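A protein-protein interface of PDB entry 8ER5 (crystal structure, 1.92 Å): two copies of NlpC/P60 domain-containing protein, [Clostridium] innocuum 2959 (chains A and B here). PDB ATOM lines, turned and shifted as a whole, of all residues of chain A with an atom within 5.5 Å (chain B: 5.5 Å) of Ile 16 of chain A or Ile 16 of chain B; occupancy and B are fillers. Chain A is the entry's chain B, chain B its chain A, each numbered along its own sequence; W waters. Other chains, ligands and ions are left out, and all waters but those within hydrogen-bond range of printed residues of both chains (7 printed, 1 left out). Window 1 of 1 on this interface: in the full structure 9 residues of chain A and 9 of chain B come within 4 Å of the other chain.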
ATOM      1  N   SER A  11     -35.405   1.136 -20.185  1.00  0.00           N
ATOM      2  CA  SER A  11     -35.048   2.541 -20.510  1.00  0.00           C
ATOM      3  C   SER A  11     -33.595   2.825 -20.103  1.00  0.00           C
ATOM      4  O   SER A  11     -32.922   3.579 -20.845  1.00  0.00           O
ATOM      5  CB  SER A  11     -36.003   3.542 -19.872  1.00  0.00           C
ATOM      6  OG  SER A  11     -35.948   3.469 -18.466  1.00  0.00           O
ATOM      7  N   SER A  12     -33.130   2.251 -18.988  1.00  0.00           N
ATOM      8  CA  SER A  12     -31.733   2.492 -18.533  1.00  0.00           C
ATOM      9  C   SER A  12     -30.738   1.835 -19.498  1.00  0.00           C
ATOM     10  O   SER A  12     -29.739   2.483 -19.833  1.00  0.00           O
ATOM     11  CB  SER A  12     -31.529   2.045 -17.107  1.00  0.00           C
ATOM     12  OG  SER A  12     -32.289   2.871 -16.230  1.00  0.00           O
ATOM     13  N   ALA A  13     -31.003   0.604 -19.934  1.00  0.00           N
ATOM     14  CA  ALA A  13     -30.099  -0.033 -20.918  1.00  0.00           C
ATOM     15  C   ALA A  13     -29.995   0.874 -22.151  1.00  0.00           C
ATOM     16  O   ALA A  13     -28.872   1.039 -22.662  1.00  0.00           O
ATOM     17  CB  ALA A  13     -30.600  -1.410 -21.289  1.00  0.00           C
ATOM     18  N   ALA A  14     -31.119   1.444 -22.603  1.00  0.00           N
ATOM     19  CA  ALA A  14     -31.091   2.327 -23.801  1.00  0.00           C
ATOM     20  C   ALA A  14     -30.179   3.531 -23.533  1.00  0.00           C
ATOM     21  O   ALA A  14     -29.365   3.859 -24.412  1.00  0.00           O
ATOM     22  CB  ALA A  14     -32.476   2.782 -24.175  1.00  0.00           C
ATOM     23  N   GLY A  15     -30.329   4.162 -22.365  1.00  0.00           N
ATOM     24  CA  GLY A  15     -29.517   5.341 -22.006  1.00  0.00           C
ATOM     25  C   GLY A  15     -28.040   5.000 -21.937  1.00  0.00           C
ATOM     26  O   GLY A  15     -27.224   5.799 -22.425  1.00  0.00           O
ATOM     27  N   ILE A  16     -27.705   3.851 -21.348  1.00  0.00           N
ATOM     28  CA  ILE A  16     -26.283   3.411 -21.264  1.00  0.00           C
ATOM     29  C   ILE A  16     -25.757   3.180 -22.688  1.00  0.00           C
ATOM     30  O   ILE A  16     -24.661   3.672 -23.003  1.00  0.00           O
ATOM     31  CB  ILE A  16     -26.158   2.160 -20.372  1.00  0.00           C
ATOM     32  CG1 ILE A  16     -26.672   2.430 -18.958  1.00  0.00           C
ATOM     33  CG2 ILE A  16     -24.720   1.662 -20.360  1.00  0.00           C
ATOM     34  CD1 ILE A  16     -26.799   1.198 -18.092  1.00  0.00           C
ATOM     35  N   ALA A  17     -26.515   2.483 -23.529  1.00  0.00           N
ATOM     36  CA  ALA A  17     -26.060   2.244 -24.921  1.00  0.00           C
ATOM     37  C   ALA A  17     -25.833   3.585 -25.639  1.00  0.00           C
ATOM     38  O   ALA A  17     -24.770   3.761 -26.280  1.00  0.00           O
ATOM     39  CB  ALA A  17     -27.068   1.398 -25.652  1.00  0.00           C
ATOM     40  N   ALA A  18     -26.790   4.508 -25.523  1.00  0.00           N
ATOM     41  CA  ALA A  18     -26.658   5.828 -26.173  1.00  0.00           C
ATOM     42  C   ALA A  18     -25.389   6.528 -25.671  1.00  0.00           C
ATOM     43  O   ALA A  18     -24.685   7.143 -26.501  1.00  0.00           O
ATOM     44  CB  ALA A  18     -27.893   6.648 -25.911  1.00  0.00           C
ATOM     45  N   SER A  19     -25.084   6.417 -24.373  1.00  0.00           N
ATOM     46  CA  SER A  19     -23.880   7.082 -23.818  1.00  0.00           C
ATOM     47  C   SER A  19     -22.606   6.435 -24.364  1.00  0.00           C
ATOM     48  O   SER A  19     -21.543   7.040 -24.280  1.00  0.00           O
ATOM     49  CB  SER A  19     -23.893   7.073 -22.303  1.00  0.00           C
ATOM     50  OG  SER A  19     -23.605   5.777 -21.799  1.00  0.00           O
ATOM     51  N   MET A  20     -22.705   5.208 -24.900  1.00  0.00           N
ATOM     52  CA  MET A  20     -21.532   4.534 -25.442  1.00  0.00           C
ATOM     53  C   MET A  20     -21.304   4.897 -26.915  1.00  0.00           C
ATOM     54  O   MET A  20     -20.345   4.415 -27.528  1.00  0.00           O
ATOM     55  CB  MET A  20     -21.668   3.015 -25.299  1.00  0.00           C
ATOM     56  CG  MET A  20     -21.546   2.501 -23.885  1.00  0.00           C
ATOM     57  SD  MET A  20     -19.818   2.980 -23.082  1.00  0.00           S
ATOM     58  CE  MET A  20     -20.256   4.172 -21.586  1.00  0.00           C
ATOM     59  N   TYR A  43     -23.498  -5.478 -22.623  1.00  0.00           N
ATOM     60  CA  TYR A  43     -22.903  -4.526 -21.658  1.00  0.00           C
ATOM     61  C   TYR A  43     -23.988  -3.578 -21.118  1.00  0.00           C
ATOM     62  O   TYR A  43     -24.079  -3.381 -19.882  1.00  0.00           O
ATOM     63  CB  TYR A  43     -21.774  -3.732 -22.311  1.00  0.00           C
ATOM     64  CG  TYR A  43     -21.227  -2.650 -21.421  1.00  0.00           C
ATOM     65  CD1 TYR A  43     -20.306  -2.943 -20.430  1.00  0.00           C
ATOM     66  CD2 TYR A  43     -21.654  -1.340 -21.541  1.00  0.00           C
ATOM     67  CE1 TYR A  43     -19.816  -1.964 -19.583  1.00  0.00           C
ATOM     68  CE2 TYR A  43     -21.170  -0.344 -20.705  1.00  0.00           C
ATOM     69  CZ  TYR A  43     -20.234  -0.655 -19.736  1.00  0.00           C
ATOM     70  OH  TYR A  43     -19.751   0.311 -18.907  1.00  0.00           O
ATOM     71  N   ALA A  44     -24.794  -3.022 -22.022  1.00  0.00           N
ATOM     72  CA  ALA A  44     -25.841  -2.039 -21.657  1.00  0.00           C
ATOM     73  C   ALA A  44     -26.821  -2.658 -20.655  1.00  0.00           C
ATOM     74  O   ALA A  44     -27.164  -1.972 -19.641  1.00  0.00           O
ATOM     75  CB  ALA A  44     -26.542  -1.566 -22.898  1.00  0.00           C
ATOM     76  N   GLN A  47     -25.115  -3.475 -17.191  1.00  0.00           N
ATOM     77  CA  GLN A  47     -24.936  -2.217 -16.413  1.00  0.00           C
ATOM     78  C   GLN A  47     -26.282  -1.742 -15.851  1.00  0.00           C
ATOM     79  O   GLN A  47     -26.256  -0.988 -14.837  1.00  0.00           O
ATOM     80  CB  GLN A  47     -24.285  -1.134 -17.279  1.00  0.00           C
ATOM     81  CG  GLN A  47     -22.828  -1.414 -17.621  1.00  0.00           C
ATOM     82  CD  GLN A  47     -21.939  -1.408 -16.403  1.00  0.00           C
ATOM     83  OE1 GLN A  47     -22.027  -0.532 -15.544  1.00  0.00           O
ATOM     84  NE2 GLN A  47     -21.043  -2.380 -16.338  1.00  0.00           N
ATOM     85  N   ALA A  48     -27.396  -2.162 -16.469  1.00  0.00           N
ATOM     86  CA  ALA A  48     -28.758  -1.839 -15.971  1.00  0.00           C
ATOM     87  C   ALA A  48     -29.242  -2.930 -15.000  1.00  0.00           C
ATOM     88  O   ALA A  48     -30.388  -2.823 -14.515  1.00  0.00           O
ATOM     89  CB  ALA A  48     -29.713  -1.673 -17.126  1.00  0.00           C
ATOM     90  N   SER B  11     -20.145   5.635 -14.915  1.00  0.00           N
ATOM     91  CA  SER B  11     -20.411   6.037 -16.322  1.00  0.00           C
ATOM     92  C   SER B  11     -21.860   5.707 -16.682  1.00  0.00           C
ATOM     93  O   SER B  11     -22.479   6.495 -17.406  1.00  0.00           O
ATOM     94  CB  SER B  11     -19.439   5.395 -17.273  1.00  0.00           C
ATOM     95  OG  SER B  11     -19.374   4.000 -17.054  1.00  0.00           O
ATOM     96  N   SER B  12     -22.383   4.608 -16.144  1.00  0.00           N
ATOM     97  CA  SER B  12     -23.778   4.184 -16.439  1.00  0.00           C
ATOM     98  C   SER B  12     -24.773   5.186 -15.831  1.00  0.00           C
ATOM     99  O   SER B  12     -25.738   5.553 -16.532  1.00  0.00           O
ATOM    100  CB  SER B  12     -24.009   2.782 -15.964  1.00  0.00           C
ATOM    101  OG  SER B  12     -23.219   1.867 -16.710  1.00  0.00           O
ATOM    102  N   ALA B  13     -24.544   5.638 -14.594  1.00  0.00           N
ATOM    103  CA  ALA B  13     -25.441   6.654 -13.986  1.00  0.00           C
ATOM    104  C   ALA B  13     -25.454   7.923 -14.856  1.00  0.00           C
ATOM    105  O   ALA B  13     -26.543   8.496 -15.060  1.00  0.00           O
ATOM    106  CB  ALA B  13     -25.004   6.945 -12.566  1.00  0.00           C
ATOM    107  N   ALA B  14     -24.288   8.341 -15.356  1.00  0.00           N
ATOM    108  CA  ALA B  14     -24.186   9.527 -16.243  1.00  0.00           C
ATOM    109  C   ALA B  14     -25.020   9.308 -17.515  1.00  0.00           C
ATOM    110  O   ALA B  14     -25.733  10.236 -17.910  1.00  0.00           O
ATOM    111  CB  ALA B  14     -22.742   9.805 -16.581  1.00  0.00           C
ATOM    112  N   GLY B  15     -24.922   8.123 -18.123  1.00  0.00           N
ATOM    113  CA  GLY B  15     -25.682   7.807 -19.345  1.00  0.00           C
ATOM    114  C   GLY B  15     -27.171   7.794 -19.074  1.00  0.00           C
ATOM    115  O   GLY B  15     -27.936   8.321 -19.907  1.00  0.00           O
ATOM    116  N   ILE B  16     -27.575   7.188 -17.957  1.00  0.00           N
ATOM    117  CA  ILE B  16     -29.022   7.133 -17.590  1.00  0.00           C
ATOM    118  C   ILE B  16     -29.530   8.563 -17.384  1.00  0.00           C
ATOM    119  O   ILE B  16     -30.580   8.900 -17.955  1.00  0.00           O
ATOM    120  CB  ILE B  16     -29.232   6.216 -16.368  1.00  0.00           C
ATOM    121  CG1 ILE B  16     -28.852   4.773 -16.720  1.00  0.00           C
ATOM    122  CG2 ILE B  16     -30.659   6.323 -15.857  1.00  0.00           C
ATOM    123  CD1 ILE B  16     -28.611   3.870 -15.532  1.00  0.00           C
ATOM    124  N   ALA B  17     -28.798   9.377 -16.618  1.00  0.00           N
ATOM    125  CA  ALA B  17     -29.207  10.775 -16.375  1.00  0.00           C
ATOM    126  C   ALA B  17     -29.313  11.524 -17.708  1.00  0.00           C
ATOM    127  O   ALA B  17     -30.344  12.172 -17.935  1.00  0.00           O
ATOM    128  CB  ALA B  17     -28.240  11.437 -15.429  1.00  0.00           C
ATOM    129  N   ALA B  18     -28.303  11.415 -18.573  1.00  0.00           N
ATOM    130  CA  ALA B  18     -28.367  12.112 -19.880  1.00  0.00           C
ATOM    131  C   ALA B  18     -29.623  11.667 -20.653  1.00  0.00           C
ATOM    132  O   ALA B  18     -30.234  12.529 -21.313  1.00  0.00           O
ATOM    133  CB  ALA B  18     -27.110  11.859 -20.668  1.00  0.00           C
ATOM    134  N   SER B  19     -29.990  10.382 -20.586  1.00  0.00           N
ATOM    135  CA  SER B  19     -31.187   9.885 -21.326  1.00  0.00           C
ATOM    136  C   SER B  19     -32.480  10.426 -20.711  1.00  0.00           C
ATOM    137  O   SER B  19     -33.530  10.317 -21.325  1.00  0.00           O
ATOM    138  CB  SER B  19     -31.223   8.378 -21.402  1.00  0.00           C
ATOM    139  OG  SER B  19     -31.621   7.817 -20.159  1.00  0.00           O
ATOM    140  N   MET B  20     -32.411  11.028 -19.513  1.00  0.00           N
ATOM    141  CA  MET B  20     -33.606  11.562 -18.881  1.00  0.00           C
ATOM    142  C   MET B  20     -33.793  13.033 -19.234  1.00  0.00           C
ATOM    143  O   MET B  20     -34.775  13.634 -18.820  1.00  0.00           O
ATOM    144  CB  MET B  20     -33.555  11.369 -17.363  1.00  0.00           C
ATOM    145  CG  MET B  20     -33.741   9.940 -16.929  1.00  0.00           C
ATOM    146  SD  MET B  20     -35.490   9.214 -17.478  1.00  0.00           S
ATOM    147  CE  MET B  20     -35.126   7.743 -18.730  1.00  0.00           C
ATOM    148  N   TYR B  43     -32.280   8.441  -8.751  1.00  0.00           N
ATOM    149  CA  TYR B  43     -32.842   7.515  -9.774  1.00  0.00           C
ATOM    150  C   TYR B  43     -31.717   6.991 -10.676  1.00  0.00           C
ATOM    151  O   TYR B  43     -31.625   5.764 -10.870  1.00  0.00           O
ATOM    152  CB  TYR B  43     -33.885   8.204 -10.657  1.00  0.00           C
ATOM    153  CG  TYR B  43     -34.375   7.373 -11.821  1.00  0.00           C
ATOM    154  CD1 TYR B  43     -35.383   6.439 -11.657  1.00  0.00           C
ATOM    155  CD2 TYR B  43     -33.869   7.548 -13.099  1.00  0.00           C
ATOM    156  CE1 TYR B  43     -35.866   5.689 -12.720  1.00  0.00           C
ATOM    157  CE2 TYR B  43     -34.331   6.798 -14.172  1.00  0.00           C
ATOM    158  CZ  TYR B  43     -35.331   5.864 -13.982  1.00  0.00           C
ATOM    159  OH  TYR B  43     -35.800   5.121 -15.033  1.00  0.00           O
ATOM    160  N   ALA B  44     -30.872   7.896 -11.178  1.00  0.00           N
ATOM    161  CA  ALA B  44     -29.787   7.485 -12.103  1.00  0.00           C
ATOM    162  C   ALA B  44     -28.913   6.421 -11.433  1.00  0.00           C
ATOM    163  O   ALA B  44     -28.589   5.400 -12.091  1.00  0.00           O
ATOM    164  CB  ALA B  44     -28.973   8.689 -12.520  1.00  0.00           C
ATOM    165  N   GLN B  47     -30.762   3.038 -10.830  1.00  0.00           N
ATOM    166  CA  GLN B  47     -30.857   2.285 -12.109  1.00  0.00           C
ATOM    167  C   GLN B  47     -29.494   1.687 -12.470  1.00  0.00           C
ATOM    168  O   GLN B  47     -29.485   0.665 -13.170  1.00  0.00           O
ATOM    169  CB  GLN B  47     -31.384   3.196 -13.208  1.00  0.00           C
ATOM    170  CG  GLN B  47     -32.843   3.565 -13.013  1.00  0.00           C
ATOM    171  CD  GLN B  47     -33.734   2.360 -13.151  1.00  0.00           C
ATOM    172  OE1 GLN B  47     -33.679   1.632 -14.139  1.00  0.00           O
ATOM    173  NE2 GLN B  47     -34.608   2.169 -12.181  1.00  0.00           N
ATOM    174  N   ALA B  48     -28.408   2.303 -11.984  1.00  0.00           N
ATOM    175  CA  ALA B  48     -27.036   1.810 -12.237  1.00  0.00           C
ATOM    176  C   ALA B  48     -26.623   0.838 -11.120  1.00  0.00           C
ATOM    177  O   ALA B  48     -25.460   0.402 -11.123  1.00  0.00           O
ATOM    178  CB  ALA B  48     -26.087   2.979 -12.366  1.00  0.00           C
HETATM  179  O   HOH W   1     -21.126   2.515 -18.533  1.00  0.00           O
HETATM  180  O   HOH W   2     -34.072   4.834 -17.042  1.00  0.00           O
HETATM  181  O   HOH W   3     -27.466   8.467 -22.583  1.00  0.00           O
HETATM  182  O   HOH W   4     -21.756   7.225 -19.978  1.00  0.00           O
HETATM  183  O   HOH W   5     -33.493   6.109 -21.434  1.00  0.00           O
HETATM  184  O   HOH W   6     -24.019  -0.022 -13.654  1.00  0.00           O
HETATM  185  O   HOH W   7     -31.841  -0.459 -14.291  1.00  0.00           O
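Among the printed residues, 12 pairs touch across the chains.
Water W5 lies within hydrogen-bond range of O of Ser 11 of chain A and OG of Ser 19 of chain B. Water W2 lies within hydrogen-bond range of OH of Tyr 43 of chain B (2.7 Å), OG of Ser 11 of chain A (2.7 Å) and OG of Ser 12 of chain A (2.8 Å). Water W3 lies within hydrogen-bond range of O of Gly 15 of chain A and O of Gly 15 of chain B. Water W6 bridges O of Gln 47 of chain A (2.7 Å) and O of Ala 48 of chain B (2.9 Å). Water W4 bridges the backbone carbonyl oxygen (O) of Ser 11 of chain B (2.8 Å) and the side-chain hydroxyl (OG) of Ser 19 of chain A (3.0 Å). Water W7 bridges the backbone carbonyl oxygen of Ala 48 of chain A and the side-chain amide oxygen of Gln 47 of chain B.
Of the printed residues of chain B, Ser 11 of chain A touches Tyr 43. Ile 16 of chain A touches two residues of chain B. Ala 18 of chain A touches none of the printed residues of chain B. Printed residues of chain B within 4 Å of Ala 48 of chain A: Gln 47 (3.8 Å). Of the printed residues of chain A, Ser 12 of chain B touches Ile 16 and Gln 47. Of chain A, only Ser 12 and Ile 16 come within 4 Å of Ile 16 of chain B. Ala 18 of chain B touches none of the printed residues of chain A. Printed residues of chain A within 4 Å of Gln 47 of chain B: Ser 12, Gln 47 and Ala 48. Printed residues of chain A within 4 Å of Ala 48 of chain B: Gln 47. The nearest residue of chain A that does not touch Ile 16 of chain B is Gly 15 of chain A (4.6 Å). The nearest printed residue of chain A that does not touch Ala 48 of chain B is Ala 48 of chain A (5.5 Å).
O of Ile 16 of chain B lies within hydrogen-bond range of OG of Ser 19 of chain B (2.7 Å). OG of Ser 19 of chain A is in hydrogen-bond range of O of Ile 16 of chain A, at 2.6 Å.
OH of Tyr 43 of chain B touches OG of Ser 11 of chain A (3.8 Å). Ile 16 of chain B touches Ser 12 of chain A (CD1 to CB, 3.8 Å). Gly 15 of chain A touches Gly 15 of chain B (O to O, 3.6 Å). CB of Ser 19 of chain B touches CA of Gly 15 of chain A, at 3.5 Å. Ser 12 of chain B touches Ile 16 of chain A (CB to CD1, 3.8 Å). Ile 16 of chain A touches Ile 16 of chain B. Gly 15 of chain B touches Ser 19 of chain A. Gln 47 of chain B touches Gln 47 of chain A (O to O, 3.99 Å). Gln 47 of chain A touches Ala 48 of chain B. CA of Ala 48 of chain A touches O of Gln 47 of chain B (3.8 Å).
Ser 11 of chain A touches Tyr 43 of chain B, but with the chains exchanged Tyr 43 of chain A does not touch Ser 11 of chain B (4.1 Å). Gly 15 of chain A touches its own counterpart, Gly 15 of chain B. Ile 16 of chain B touches its own counterpart, Ile 16 of chain A. Gln 47 of chain A touches its own counterpart, Gln 47 of chain B. 14 positions are printed for both chains.
OG of Ser 12 of chain B sits at hydrogen-bond distance from OE1 of Gln 47 of chain A (2.9 Å). The side-chain amide oxygen (OE1) of Gln 47 of chain B is in hydrogen-bond range of the side-chain hydroxyl (OG) of Ser 12 of chain A (2.8 Å).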
